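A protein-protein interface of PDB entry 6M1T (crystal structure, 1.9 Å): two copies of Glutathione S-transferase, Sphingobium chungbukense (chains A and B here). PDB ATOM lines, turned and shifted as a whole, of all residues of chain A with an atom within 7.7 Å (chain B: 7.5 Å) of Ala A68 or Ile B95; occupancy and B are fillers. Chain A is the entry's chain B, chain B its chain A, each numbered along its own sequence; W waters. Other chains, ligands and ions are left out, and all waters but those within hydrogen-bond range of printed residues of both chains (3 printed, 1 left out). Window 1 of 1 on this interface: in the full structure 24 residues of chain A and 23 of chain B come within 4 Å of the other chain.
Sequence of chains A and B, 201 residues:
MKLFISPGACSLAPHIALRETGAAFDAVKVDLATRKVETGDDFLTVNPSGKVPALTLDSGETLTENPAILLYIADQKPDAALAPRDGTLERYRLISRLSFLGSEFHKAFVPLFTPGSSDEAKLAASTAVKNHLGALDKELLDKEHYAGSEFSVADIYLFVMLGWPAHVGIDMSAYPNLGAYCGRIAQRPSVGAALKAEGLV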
ATOM      1  N   LEU A  55     -19.980  -6.694   5.099  1.00  0.00           N
ATOM      2  CA  LEU A  55     -18.589  -6.998   5.485  1.00  0.00           C
ATOM      3  C   LEU A  55     -17.997  -5.713   6.052  1.00  0.00           C
ATOM      4  O   LEU A  55     -17.840  -4.715   5.280  1.00  0.00           O
ATOM      5  CB  LEU A  55     -17.766  -7.520   4.306  1.00  0.00           C
ATOM      6  CG  LEU A  55     -16.334  -7.961   4.661  1.00  0.00           C
ATOM      7  CD1 LEU A  55     -16.321  -9.148   5.607  1.00  0.00           C
ATOM      8  CD2 LEU A  55     -15.518  -8.301   3.429  1.00  0.00           C
ATOM      9  N   LEU A  63     -18.684  -2.814   3.425  1.00  0.00           N
ATOM     10  CA  LEU A  63     -19.038  -3.165   2.014  1.00  0.00           C
ATOM     11  C   LEU A  63     -20.348  -3.944   2.038  1.00  0.00           C
ATOM     12  O   LEU A  63     -20.482  -4.851   2.879  1.00  0.00           O
ATOM     13  CB  LEU A  63     -17.973  -4.054   1.376  1.00  0.00           C
ATOM     14  CG  LEU A  63     -16.622  -3.429   1.044  1.00  0.00           C
ATOM     15  CD1 LEU A  63     -15.787  -4.430   0.248  1.00  0.00           C
ATOM     16  CD2 LEU A  63     -16.798  -2.132   0.279  1.00  0.00           C
ATOM     17  N   THR A  64     -21.254  -3.597   1.138  1.00  0.00           N
ATOM     18  CA  THR A  64     -22.439  -4.405   0.827  1.00  0.00           C
ATOM     19  C   THR A  64     -22.384  -4.898  -0.627  1.00  0.00           C
ATOM     20  O   THR A  64     -21.574  -4.357  -1.428  1.00  0.00           O
ATOM     21  CB  THR A  64     -23.701  -3.606   1.132  1.00  0.00           C
ATOM     22  OG1 THR A  64     -23.744  -2.455   0.285  1.00  0.00           O
ATOM     23  CG2 THR A  64     -23.777  -3.208   2.591  1.00  0.00           C
ATOM     24  N   GLU A  65     -23.320  -5.809  -0.955  1.00  0.00           N
ATOM     25  CA  GLU A  65     -23.532  -6.371  -2.318  1.00  0.00           C
ATOM     26  C   GLU A  65     -22.532  -7.499  -2.518  1.00  0.00           C
ATOM     27  O   GLU A  65     -21.277  -7.260  -2.544  1.00  0.00           O
ATOM     28  CB  GLU A  65     -23.394  -5.293  -3.402  1.00  0.00           C
ATOM     29  CG  GLU A  65     -24.453  -4.223  -3.354  1.00  0.00           C
ATOM     30  CD  GLU A  65     -25.897  -4.674  -3.537  1.00  0.00           C
ATOM     31  OE1 GLU A  65     -26.774  -4.088  -2.849  1.00  0.00           O
ATOM     32  OE2 GLU A  65     -26.167  -5.584  -4.389  1.00  0.00           O
ATOM     33  N   ASN A  66     -23.045  -8.705  -2.695  1.00  0.00           N
ATOM     34  CA  ASN A  66     -22.224  -9.913  -2.884  1.00  0.00           C
ATOM     35  C   ASN A  66     -21.105  -9.695  -3.897  1.00  0.00           C
ATOM     36  O   ASN A  66     -19.953 -10.045  -3.581  1.00  0.00           O
ATOM     37  CB  ASN A  66     -23.081 -11.142  -3.201  1.00  0.00           C
ATOM     38  CG  ASN A  66     -23.145 -12.077  -2.013  1.00  0.00           C
ATOM     39  OD1 ASN A  66     -22.139 -12.304  -1.348  1.00  0.00           O
ATOM     40  ND2 ASN A  66     -24.320 -12.590  -1.738  1.00  0.00           N
ATOM     41  N   PRO A  67     -21.365  -9.220  -5.142  1.00  0.00           N
ATOM     42  CA  PRO A  67     -20.305  -9.114  -6.139  1.00  0.00           C
ATOM     43  C   PRO A  67     -19.096  -8.318  -5.598  1.00  0.00           C
ATOM     44  O   PRO A  67     -17.976  -8.737  -5.810  1.00  0.00           O
ATOM     45  CB  PRO A  67     -21.014  -8.462  -7.347  1.00  0.00           C
ATOM     46  CG  PRO A  67     -22.457  -8.907  -7.182  1.00  0.00           C
ATOM     47  CD  PRO A  67     -22.711  -8.874  -5.688  1.00  0.00           C
ATOM     48  N   ALA A  68     -19.352  -7.277  -4.842  1.00  0.00           N
ATOM     49  CA  ALA A  68     -18.291  -6.377  -4.322  1.00  0.00           C
ATOM     50  C   ALA A  68     -17.559  -7.095  -3.185  1.00  0.00           C
ATOM     51  O   ALA A  68     -16.312  -7.090  -3.163  1.00  0.00           O
ATOM     52  CB  ALA A  68     -18.879  -5.093  -3.885  1.00  0.00           C
ATOM     53  N   ILE A  69     -18.330  -7.665  -2.257  1.00  0.00           N
ATOM     54  CA  ILE A  69     -17.782  -8.336  -1.046  1.00  0.00           C
ATOM     55  C   ILE A  69     -16.918  -9.499  -1.513  1.00  0.00           C
ATOM     56  O   ILE A  69     -15.793  -9.690  -1.000  1.00  0.00           O
ATOM     57  CB  ILE A  69     -18.914  -8.768  -0.103  1.00  0.00           C
ATOM     58  CG1 ILE A  69     -19.597  -7.558   0.522  1.00  0.00           C
ATOM     59  CG2 ILE A  69     -18.353  -9.768   0.908  1.00  0.00           C
ATOM     60  CD1 ILE A  69     -20.960  -7.816   1.094  1.00  0.00           C
ATOM     61  N   LEU A  70     -17.410 -10.278  -2.479  1.00  0.00           N
ATOM     62  CA  LEU A  70     -16.738 -11.479  -2.992  1.00  0.00           C
ATOM     63  C   LEU A  70     -15.430 -11.110  -3.703  1.00  0.00           C
ATOM     64  O   LEU A  70     -14.409 -11.815  -3.478  1.00  0.00           O
ATOM     65  CB  LEU A  70     -17.692 -12.224  -3.930  1.00  0.00           C
ATOM     66  CG  LEU A  70     -18.795 -13.019  -3.219  1.00  0.00           C
ATOM     67  CD1 LEU A  70     -19.726 -13.613  -4.270  1.00  0.00           C
ATOM     68  CD2 LEU A  70     -18.235 -14.112  -2.314  1.00  0.00           C
ATOM     69  N   LEU A  71     -15.413 -10.031  -4.472  1.00  0.00           N
ATOM     70  CA  LEU A  71     -14.135  -9.618  -5.142  1.00  0.00           C
ATOM     71  C   LEU A  71     -13.114  -9.118  -4.103  1.00  0.00           C
ATOM     72  O   LEU A  71     -11.940  -9.500  -4.198  1.00  0.00           O
ATOM     73  CB  LEU A  71     -14.440  -8.556  -6.197  1.00  0.00           C
ATOM     74  CG  LEU A  71     -15.144  -9.099  -7.440  1.00  0.00           C
ATOM     75  CD1 LEU A  71     -15.506  -7.985  -8.390  1.00  0.00           C
ATOM     76  CD2 LEU A  71     -14.326 -10.128  -8.186  1.00  0.00           C
ATOM     77  N   TYR A  72     -13.554  -8.319  -3.152  1.00  0.00           N
ATOM     78  CA  TYR A  72     -12.725  -7.854  -2.003  1.00  0.00           C
ATOM     79  C   TYR A  72     -12.067  -9.062  -1.301  1.00  0.00           C
ATOM     80  O   TYR A  72     -10.828  -9.076  -1.087  1.00  0.00           O
ATOM     81  CB  TYR A  72     -13.545  -7.006  -1.039  1.00  0.00           C
ATOM     82  CG  TYR A  72     -12.727  -6.550   0.149  1.00  0.00           C
ATOM     83  CD1 TYR A  72     -12.546  -7.381   1.247  1.00  0.00           C
ATOM     84  CD2 TYR A  72     -12.036  -5.352   0.120  1.00  0.00           C
ATOM     85  CE1 TYR A  72     -11.778  -6.984   2.326  1.00  0.00           C
ATOM     86  CE2 TYR A  72     -11.228  -4.956   1.176  1.00  0.00           C
ATOM     87  CZ  TYR A  72     -11.093  -5.780   2.276  1.00  0.00           C
ATOM     88  OH  TYR A  72     -10.306  -5.398   3.326  1.00  0.00           O
ATOM     89  N   ILE A  73     -12.854 -10.076  -0.949  1.00  0.00           N
ATOM     90  CA  ILE A  73     -12.360 -11.302  -0.252  1.00  0.00           C
ATOM     91  C   ILE A  73     -11.282 -11.979  -1.114  1.00  0.00           C
ATOM     92  O   ILE A  73     -10.173 -12.289  -0.572  1.00  0.00           O
ATOM     93  CB  ILE A  73     -13.514 -12.250   0.124  1.00  0.00           C
ATOM     94  CG1 ILE A  73     -14.393 -11.640   1.215  1.00  0.00           C
ATOM     95  CG2 ILE A  73     -12.995 -13.629   0.506  1.00  0.00           C
ATOM     96  CD1 ILE A  73     -15.725 -12.335   1.391  1.00  0.00           C
ATOM     97  N   ALA A  74     -11.573 -12.227  -2.395  1.00  0.00           N
ATOM     98  CA  ALA A  74     -10.640 -12.860  -3.347  1.00  0.00           C
ATOM     99  C   ALA A  74      -9.323 -12.053  -3.397  1.00  0.00           C
ATOM    100  O   ALA A  74      -8.224 -12.690  -3.361  1.00  0.00           O
ATOM    101  CB  ALA A  74     -11.275 -12.957  -4.717  1.00  0.00           C
ATOM    102  N   ASP A  75      -9.419 -10.730  -3.477  1.00  0.00           N
ATOM    103  CA  ASP A  75      -8.243  -9.855  -3.749  1.00  0.00           C
ATOM    104  C   ASP A  75      -7.446  -9.576  -2.464  1.00  0.00           C
ATOM    105  O   ASP A  75      -6.370  -9.015  -2.587  1.00  0.00           O
ATOM    106  CB  ASP A  75      -8.647  -8.509  -4.309  1.00  0.00           C
ATOM    107  CG  ASP A  75      -9.362  -8.543  -5.651  1.00  0.00           C
ATOM    108  OD1 ASP A  75      -9.237  -9.564  -6.336  1.00  0.00           O
ATOM    109  OD2 ASP A  75     -10.020  -7.499  -5.975  1.00  0.00           O
ATOM    110  N   ASP A  86      -7.198  -7.805 -11.551  1.00  0.00           N
ATOM    111  CA  ASP A  86      -8.079  -6.687 -11.992  1.00  0.00           C
ATOM    112  C   ASP A  86      -7.504  -6.154 -13.324  1.00  0.00           C
ATOM    113  O   ASP A  86      -6.275  -6.179 -13.524  1.00  0.00           O
ATOM    114  CB  ASP A  86      -8.263  -5.651 -10.866  1.00  0.00           C
ATOM    115  CG  ASP A  86      -9.566  -4.838 -10.884  1.00  0.00           C
ATOM    116  OD1 ASP A  86     -10.357  -5.010 -11.836  1.00  0.00           O
ATOM    117  OD2 ASP A  86      -9.795  -4.017  -9.929  1.00  0.00           O
ATOM    118  N   ARG A  91     -11.138 -10.820 -15.716  1.00  0.00           N
ATOM    119  CA  ARG A  91     -11.761 -10.076 -14.591  1.00  0.00           C
ATOM    120  C   ARG A  91     -13.159  -9.602 -15.010  1.00  0.00           C
ATOM    121  O   ARG A  91     -14.116  -9.797 -14.233  1.00  0.00           O
ATOM    122  CB  ARG A  91     -10.878  -8.902 -14.179  1.00  0.00           C
ATOM    123  CG  ARG A  91     -11.404  -8.176 -12.958  1.00  0.00           C
ATOM    124  CD  ARG A  91     -11.198  -8.986 -11.690  1.00  0.00           C
ATOM    125  NE  ARG A  91     -11.411  -8.110 -10.559  1.00  0.00           N
ATOM    126  CZ  ARG A  91     -10.941  -8.304  -9.337  1.00  0.00           C
ATOM    127  NH1 ARG A  91     -10.216  -9.367  -9.078  1.00  0.00           N
ATOM    128  NH2 ARG A  91     -11.227  -7.438  -8.384  1.00  0.00           N
ATOM    129  N   ILE A  95     -16.851 -10.539 -13.521  1.00  0.00           N
ATOM    130  CA  ILE A  95     -17.793  -9.496 -13.031  1.00  0.00           C
ATOM    131  C   ILE A  95     -19.135  -9.652 -13.761  1.00  0.00           C
ATOM    132  O   ILE A  95     -20.206  -9.568 -13.078  1.00  0.00           O
ATOM    133  CB  ILE A  95     -17.187  -8.086 -13.137  1.00  0.00           C
ATOM    134  CG1 ILE A  95     -16.021  -7.890 -12.170  1.00  0.00           C
ATOM    135  CG2 ILE A  95     -18.250  -7.010 -12.942  1.00  0.00           C
ATOM    136  CD1 ILE A  95     -15.291  -6.568 -12.391  1.00  0.00           C
ATOM    137  N   LEU A  98     -20.872 -12.682 -12.034  1.00  0.00           N
ATOM    138  CA  LEU A  98     -21.342 -12.251 -10.694  1.00  0.00           C
ATOM    139  C   LEU A  98     -22.569 -11.344 -10.845  1.00  0.00           C
ATOM    140  O   LEU A  98     -23.488 -11.556 -10.091  1.00  0.00           O
ATOM    141  CB  LEU A  98     -20.256 -11.529  -9.918  1.00  0.00           C
ATOM    142  CG  LEU A  98     -19.019 -12.353  -9.513  1.00  0.00           C
ATOM    143  CD1 LEU A  98     -18.063 -11.423  -8.800  1.00  0.00           C
ATOM    144  CD2 LEU A  98     -19.396 -13.502  -8.603  1.00  0.00           C
ATOM    145  N   PRO B  67     -22.797  -3.710 -15.105  1.00  0.00           N
ATOM    146  CA  PRO B  67     -21.657  -3.547 -14.201  1.00  0.00           C
ATOM    147  C   PRO B  67     -20.299  -3.914 -14.821  1.00  0.00           C
ATOM    148  O   PRO B  67     -19.293  -3.150 -14.640  1.00  0.00           O
ATOM    149  CB  PRO B  67     -22.053  -4.459 -13.027  1.00  0.00           C
ATOM    150  CG  PRO B  67     -23.549  -4.411 -13.006  1.00  0.00           C
ATOM    151  CD  PRO B  67     -23.929  -4.436 -14.480  1.00  0.00           C
ATOM    152  N   LEU B  71     -17.545  -0.934 -16.203  1.00  0.00           N
ATOM    153  CA  LEU B  71     -16.138  -0.990 -15.697  1.00  0.00           C
ATOM    154  C   LEU B  71     -15.145  -1.131 -16.853  1.00  0.00           C
ATOM    155  O   LEU B  71     -14.125  -0.423 -16.830  1.00  0.00           O
ATOM    156  CB  LEU B  71     -15.950  -2.155 -14.724  1.00  0.00           C
ATOM    157  CG  LEU B  71     -15.735  -1.854 -13.242  1.00  0.00           C
ATOM    158  CD1 LEU B  71     -15.326  -0.424 -12.915  1.00  0.00           C
ATOM    159  CD2 LEU B  71     -16.983  -2.241 -12.465  1.00  0.00           C
ATOM    160  N   PRO B  84     -12.498   4.237 -10.079  1.00  0.00           N
ATOM    161  CA  PRO B  84     -11.257   4.264  -9.302  1.00  0.00           C
ATOM    162  C   PRO B  84     -10.237   3.214  -9.735  1.00  0.00           C
ATOM    163  O   PRO B  84     -10.580   2.208 -10.307  1.00  0.00           O
ATOM    164  CB  PRO B  84     -11.758   3.978  -7.867  1.00  0.00           C
ATOM    165  CG  PRO B  84     -13.165   4.529  -7.844  1.00  0.00           C
ATOM    166  CD  PRO B  84     -13.687   4.127  -9.213  1.00  0.00           C
ATOM    167  N   LEU B  89     -10.146   1.085  -1.938  1.00  0.00           N
ATOM    168  CA  LEU B  89     -11.469   0.802  -1.344  1.00  0.00           C
ATOM    169  C   LEU B  89     -12.537   1.377  -2.273  1.00  0.00           C
ATOM    170  O   LEU B  89     -13.626   0.791  -2.366  1.00  0.00           O
ATOM    171  CB  LEU B  89     -11.619   1.432   0.037  1.00  0.00           C
ATOM    172  CG  LEU B  89     -12.959   1.062   0.667  1.00  0.00           C
ATOM    173  CD1 LEU B  89     -13.135  -0.473   0.648  1.00  0.00           C
ATOM    174  CD2 LEU B  89     -13.095   1.635   2.054  1.00  0.00           C
ATOM    175  N   GLU B  90     -12.258   2.523  -2.890  1.00  0.00           N
ATOM    176  CA  GLU B  90     -13.274   3.252  -3.701  1.00  0.00           C
ATOM    177  C   GLU B  90     -13.685   2.354  -4.881  1.00  0.00           C
ATOM    178  O   GLU B  90     -14.849   2.434  -5.285  1.00  0.00           O
ATOM    179  CB  GLU B  90     -12.762   4.612  -4.185  1.00  0.00           C
ATOM    180  CG  GLU B  90     -12.590   5.639  -3.082  1.00  0.00           C
ATOM    181  CD  GLU B  90     -11.391   5.440  -2.155  1.00  0.00           C
ATOM    182  OE1 GLU B  90     -10.396   4.780  -2.553  1.00  0.00           O
ATOM    183  OE2 GLU B  90     -11.475   5.925  -1.001  1.00  0.00           O
ATOM    184  N   ARG B  91     -12.793   1.506  -5.379  1.00  0.00           N
ATOM    185  CA  ARG B  91     -13.094   0.603  -6.517  1.00  0.00           C
ATOM    186  C   ARG B  91     -14.140  -0.437  -6.068  1.00  0.00           C
ATOM    187  O   ARG B  91     -15.028  -0.778  -6.877  1.00  0.00           O
ATOM    188  CB  ARG B  91     -11.833  -0.106  -6.986  1.00  0.00           C
ATOM    189  CG  ARG B  91     -12.050  -1.000  -8.190  1.00  0.00           C
ATOM    190  CD  ARG B  91     -11.048  -0.734  -9.269  1.00  0.00           C
ATOM    191  NE  ARG B  91     -11.130  -1.664 -10.377  1.00  0.00           N
ATOM    192  CZ  ARG B  91     -11.386  -1.327 -11.643  1.00  0.00           C
ATOM    193  NH1 ARG B  91     -11.627  -0.065 -11.960  1.00  0.00           N
ATOM    194  NH2 ARG B  91     -11.395  -2.267 -12.576  1.00  0.00           N
ATOM    195  N   TYR B  92     -14.054  -0.928  -4.836  1.00  0.00           N
ATOM    196  CA  TYR B  92     -15.051  -1.924  -4.332  1.00  0.00           C
ATOM    197  C   TYR B  92     -16.352  -1.191  -4.047  1.00  0.00           C
ATOM    198  O   TYR B  92     -17.412  -1.793  -4.292  1.00  0.00           O
ATOM    199  CB  TYR B  92     -14.534  -2.712  -3.135  1.00  0.00           C
ATOM    200  CG  TYR B  92     -13.290  -3.453  -3.495  1.00  0.00           C
ATOM    201  CD1 TYR B  92     -13.363  -4.691  -4.096  1.00  0.00           C
ATOM    202  CD2 TYR B  92     -12.049  -2.876  -3.293  1.00  0.00           C
ATOM    203  CE1 TYR B  92     -12.228  -5.376  -4.470  1.00  0.00           C
ATOM    204  CE2 TYR B  92     -10.900  -3.543  -3.662  1.00  0.00           C
ATOM    205  CZ  TYR B  92     -10.988  -4.789  -4.230  1.00  0.00           C
ATOM    206  OH  TYR B  92      -9.863  -5.408  -4.599  1.00  0.00           O
ATOM    207  N   ARG B  93     -16.298   0.058  -3.567  1.00  0.00           N
ATOM    208  CA  ARG B  93     -17.524   0.840  -3.273  1.00  0.00           C
ATOM    209  C   ARG B  93     -18.244   1.125  -4.597  1.00  0.00           C
ATOM    210  O   ARG B  93     -19.478   1.106  -4.588  1.00  0.00           O
ATOM    211  CB  ARG B  93     -17.241   2.139  -2.514  1.00  0.00           C
ATOM    212  CG  ARG B  93     -16.523   1.874  -1.198  1.00  0.00           C
ATOM    213  CD  ARG B  93     -16.661   2.956  -0.135  1.00  0.00           C
ATOM    214  NE  ARG B  93     -17.810   2.916   0.767  1.00  0.00           N
ATOM    215  CZ  ARG B  93     -18.409   1.828   1.282  1.00  0.00           C
ATOM    216  NH1 ARG B  93     -19.450   1.974   2.084  1.00  0.00           N
ATOM    217  NH2 ARG B  93     -18.017   0.600   0.999  1.00  0.00           N
ATOM    218  N   LEU B  94     -17.493   1.336  -5.687  1.00  0.00           N
ATOM    219  CA  LEU B  94     -18.074   1.516  -7.054  1.00  0.00           C
ATOM    220  C   LEU B  94     -18.787   0.224  -7.481  1.00  0.00           C
ATOM    221  O   LEU B  94     -19.939   0.286  -7.913  1.00  0.00           O
ATOM    222  CB  LEU B  94     -16.992   1.832  -8.087  1.00  0.00           C
ATOM    223  CG  LEU B  94     -17.549   1.899  -9.517  1.00  0.00           C
ATOM    224  CD1 LEU B  94     -18.631   2.931  -9.562  1.00  0.00           C
ATOM    225  CD2 LEU B  94     -16.503   2.187 -10.576  1.00  0.00           C
ATOM    226  N   ILE B  95     -18.109  -0.909  -7.404  1.00  0.00           N
ATOM    227  CA  ILE B  95     -18.724  -2.206  -7.807  1.00  0.00           C
ATOM    228  C   ILE B  95     -19.995  -2.452  -6.969  1.00  0.00           C
ATOM    229  O   ILE B  95     -21.039  -2.982  -7.516  1.00  0.00           O
ATOM    230  CB  ILE B  95     -17.670  -3.307  -7.689  1.00  0.00           C
ATOM    231  CG1 ILE B  95     -16.510  -3.061  -8.655  1.00  0.00           C
ATOM    232  CG2 ILE B  95     -18.274  -4.690  -7.897  1.00  0.00           C
ATOM    233  CD1 ILE B  95     -15.337  -3.989  -8.429  1.00  0.00           C
ATOM    234  N   SER B  96     -19.949  -2.100  -5.688  1.00  0.00           N
ATOM    235  CA  SER B  96     -21.087  -2.169  -4.736  1.00  0.00           C
ATOM    236  C   SER B  96     -22.244  -1.349  -5.292  1.00  0.00           C
ATOM    237  O   SER B  96     -23.397  -1.872  -5.427  1.00  0.00           O
ATOM    238  CB  SER B  96     -20.685  -1.689  -3.344  1.00  0.00           C
ATOM    239  OG  SER B  96     -21.767  -1.768  -2.438  1.00  0.00           O
ATOM    240  N   ARG B  97     -21.966  -0.098  -5.657  1.00  0.00           N
ATOM    241  CA  ARG B  97     -23.039   0.768  -6.177  1.00  0.00           C
ATOM    242  C   ARG B  97     -23.565   0.166  -7.498  1.00  0.00           C
ATOM    243  O   ARG B  97     -24.783   0.231  -7.706  1.00  0.00           O
ATOM    244  CB  ARG B  97     -22.585   2.233  -6.271  1.00  0.00           C
ATOM    245  CG  ARG B  97     -22.511   2.996  -4.941  1.00  0.00           C
ATOM    246  CD  ARG B  97     -23.691   2.862  -3.976  1.00  0.00           C
ATOM    247  NE  ARG B  97     -23.599   1.611  -3.214  1.00  0.00           N
ATOM    248  CZ  ARG B  97     -24.597   0.973  -2.575  1.00  0.00           C
ATOM    249  NH1 ARG B  97     -24.320  -0.161  -1.975  1.00  0.00           N
ATOM    250  NH2 ARG B  97     -25.831   1.445  -2.505  1.00  0.00           N
ATOM    251  N   LEU B  98     -22.699  -0.335  -8.382  1.00  0.00           N
ATOM    252  CA  LEU B  98     -23.193  -0.889  -9.680  1.00  0.00           C
ATOM    253  C   LEU B  98     -24.065  -2.123  -9.406  1.00  0.00           C
ATOM    254  O   LEU B  98     -25.099  -2.277 -10.127  1.00  0.00           O
ATOM    255  CB  LEU B  98     -22.024  -1.198 -10.613  1.00  0.00           C
ATOM    256  CG  LEU B  98     -21.150   0.012 -11.010  1.00  0.00           C
ATOM    257  CD1 LEU B  98     -19.994  -0.463 -11.850  1.00  0.00           C
ATOM    258  CD2 LEU B  98     -21.986   1.082 -11.735  1.00  0.00           C
ATOM    259  N   SER B  99     -23.686  -2.970  -8.436  1.00  0.00           N
ATOM    260  CA  SER B  99     -24.446  -4.211  -8.084  1.00  0.00           C
ATOM    261  C   SER B  99     -25.792  -3.797  -7.482  1.00  0.00           C
ATOM    262  O   SER B  99     -26.825  -4.394  -7.844  1.00  0.00           O
ATOM    263  CB  SER B  99     -23.658  -5.234  -7.203  1.00  0.00           C
ATOM    264  OG  SER B  99     -24.793  -5.993  -6.760  1.00  0.00           O
ATOM    265  N   PHE B 100     -25.837  -2.751  -6.648  1.00  0.00           N
ATOM    266  CA  PHE B 100     -27.105  -2.280  -6.072  1.00  0.00           C
ATOM    267  C   PHE B 100     -28.037  -1.765  -7.189  1.00  0.00           C
ATOM    268  O   PHE B 100     -29.268  -2.059  -7.187  1.00  0.00           O
ATOM    269  CB  PHE B 100     -26.878  -1.168  -5.047  1.00  0.00           C
ATOM    270  CG  PHE B 100     -28.154  -0.537  -4.625  1.00  0.00           C
ATOM    271  CD1 PHE B 100     -28.926  -1.082  -3.615  1.00  0.00           C
ATOM    272  CD2 PHE B 100     -28.563   0.645  -5.218  1.00  0.00           C
ATOM    273  CE1 PHE B 100     -30.110  -0.472  -3.212  1.00  0.00           C
ATOM    274  CE2 PHE B 100     -29.752   1.242  -4.833  1.00  0.00           C
ATOM    275  CZ  PHE B 100     -30.518   0.700  -3.819  1.00  0.00           C
ATOM    276  N   LEU B 101     -27.496  -0.986  -8.128  1.00  0.00           N
ATOM    277  CA  LEU B 101     -28.333  -0.417  -9.208  1.00  0.00           C
ATOM    278  C   LEU B 101     -28.916  -1.550 -10.094  1.00  0.00           C
ATOM    279  O   LEU B 101     -30.091  -1.481 -10.389  1.00  0.00           O
ATOM    280  CB  LEU B 101     -27.473   0.550 -10.014  1.00  0.00           C
ATOM    281  CG  LEU B 101     -27.103   1.833  -9.257  1.00  0.00           C
ATOM    282  CD1 LEU B 101     -26.159   2.686 -10.093  1.00  0.00           C
ATOM    283  CD2 LEU B 101     -28.334   2.594  -8.902  1.00  0.00           C
ATOM    284  N   ALA B 147     -20.765   7.648  -6.083  1.00  0.00           N
ATOM    285  CA  ALA B 147     -19.619   6.805  -5.641  1.00  0.00           C
ATOM    286  C   ALA B 147     -18.305   7.613  -5.601  1.00  0.00           C
ATOM    287  O   ALA B 147     -17.857   8.148  -6.666  1.00  0.00           O
ATOM    288  CB  ALA B 147     -19.479   5.594  -6.546  1.00  0.00           C
ATOM    289  N   ALA B 154     -21.075   4.940 -12.103  1.00  0.00           N
ATOM    290  CA  ALA B 154     -22.196   4.711 -11.166  1.00  0.00           C
ATOM    291  C   ALA B 154     -23.163   5.876 -11.286  1.00  0.00           C
ATOM    292  O   ALA B 154     -24.371   5.634 -11.231  1.00  0.00           O
ATOM    293  CB  ALA B 154     -21.704   4.518  -9.746  1.00  0.00           C
HETATM  294  O   HOH W   1     -26.088  -2.490  -1.031  1.00  0.00           O
HETATM  295  O   HOH W   2     -20.673  -0.924   0.050  1.00  0.00           O
HETATM  296  O   HOH W   3      -9.137  -4.049  -7.499  1.00  0.00           O
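The guanidinium group (NE) of Arg B91 lies within salt-bridge range of the side-chain carboxylate (OD2) of Asp A86 (2.7 Å).
The side-chain carboxylate of Asp A75 lies within hydrogen-bond range of the side-chain hydroxyl of Tyr B92.
O of Thr A64 sits at hydrogen-bond distance from OG of Ser B96, 2.8 Å away.
The guanidinium group (NH1) of Arg B97 sits at hydrogen-bond distance from the side-chain hydroxyl (OG1) of Thr A64 (3.3 Å).
The side-chain hydroxyl of Ser B99 lies within hydrogen-bond range of the side-chain carboxylate of Glu A65, 2.8 Å away.
The guanidinium group (NH1) of Arg B91 sits at hydrogen-bond distance from the backbone carbonyl oxygen (O) of Pro B84, 3.0 Å away.
NH1 of Arg B97 sits at hydrogen-bond distance from OG of Ser B96.
The backbone carbonyl oxygen (O) of Leu A55 is in hydrogen-bond range of the backbone NH (N) of Leu A63.
The side-chain carboxylate (OD2) of Asp A75 lies within salt-bridge range of the guanidinium group (NH2) of Arg A91.
OD1 of Asp A86 lies within salt-bridge range of NE of Arg A91.
Tyr B92 touches Leu A63.
Leu A63 touches Arg B93 (CD2 to NH2, 3.1 Å).
Ser B96 touches Glu A65 (O to CG, 3.3 Å).
OE2 of Glu A65 touches N of Phe B100, 3.6 Å away.
Ser B99 touches Pro A67 (OG to CD, 3.7 Å).
Ala A68 touches Tyr B92 (CB to O, 3.6 Å).
CA of Ala A68 touches CG2 of Ile B95 (3.95 Å).
CE1 of Tyr B92 touches C of Leu A71, 3.9 Å away.
Leu A71 touches Ile B95.
Tyr B92 touches Tyr A72 (CE1 to N, 3.5 Å).
Of the printed residues of chain B, Ala A68 touches Tyr B92 (3.6 Å), Ile B95 (3.95 Å) and Ser B96 (3.7 Å).
Of the printed residues of chain A, Ile B95 touches Ala A68 and Leu A71.
Of the printed residues of chain B, Leu A71 touches Tyr B92 (3.9 Å) and Ile B95 (3.9998 Å).
Of the printed residues of chain B, Leu A63 touches Tyr B92 and Arg B93.
Printed residues of chain A within 4 Å of Ser B99: Glu A65 and Pro A67.
Printed residues of chain B within 4 Å of Asp A75: Tyr B92 (2.5 Å).
Leu A70 touches none of the printed residues of chain B.
Pro B84 touches none of the printed residues of chain A.
The nearest printed residue of chain A that does not touch Ile B95 is Pro A67 (4.4 Å).
Of the 18 printed residues of chain A, 9 touch a printed residue of chain B.
Printed residues of chain A that touch a printed residue of chain B: Leu A63, Thr A64, Glu A65, Pro A67, Ala A68, Leu A71, Tyr A72, Asp A75 and Asp A86.
Hydrophobic or aromatic side chains of chain A within 4 Å of the printed part of chain B: Leu A63, Pro A67, Ala A68, Leu A71 and Tyr A72.
Of the 18 printed residues of chain B, 8 touch a printed residue of chain A.
Among the printed residues, Asp or Glu carboxylates within 4 Å of a Lys or Arg side-chain nitrogen of the other chain: Asp A86 with Arg B91.
Leu A71 touches Ile B95, but with the chains exchanged Ile A95 does not touch Leu B71 (4.6 Å).
Positions printed for both chains: 67, 71, 91, 95 and 98.
Water W1 lies within hydrogen-bond range of OE1 of Glu A65 (2.5 Å), OG1 of Thr A64 (2.7 Å) and NH1 of Arg B97 (3.1 Å).
Water W3 lies within hydrogen-bond range of OD2 of Asp A86 and OH of Tyr B92.
Water W2 lies within hydrogen-bond range of OG of Ser B96 (2.8 Å), N of Thr A64 (2.9 Å) and NH2 of Arg B93 (3.2 Å).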
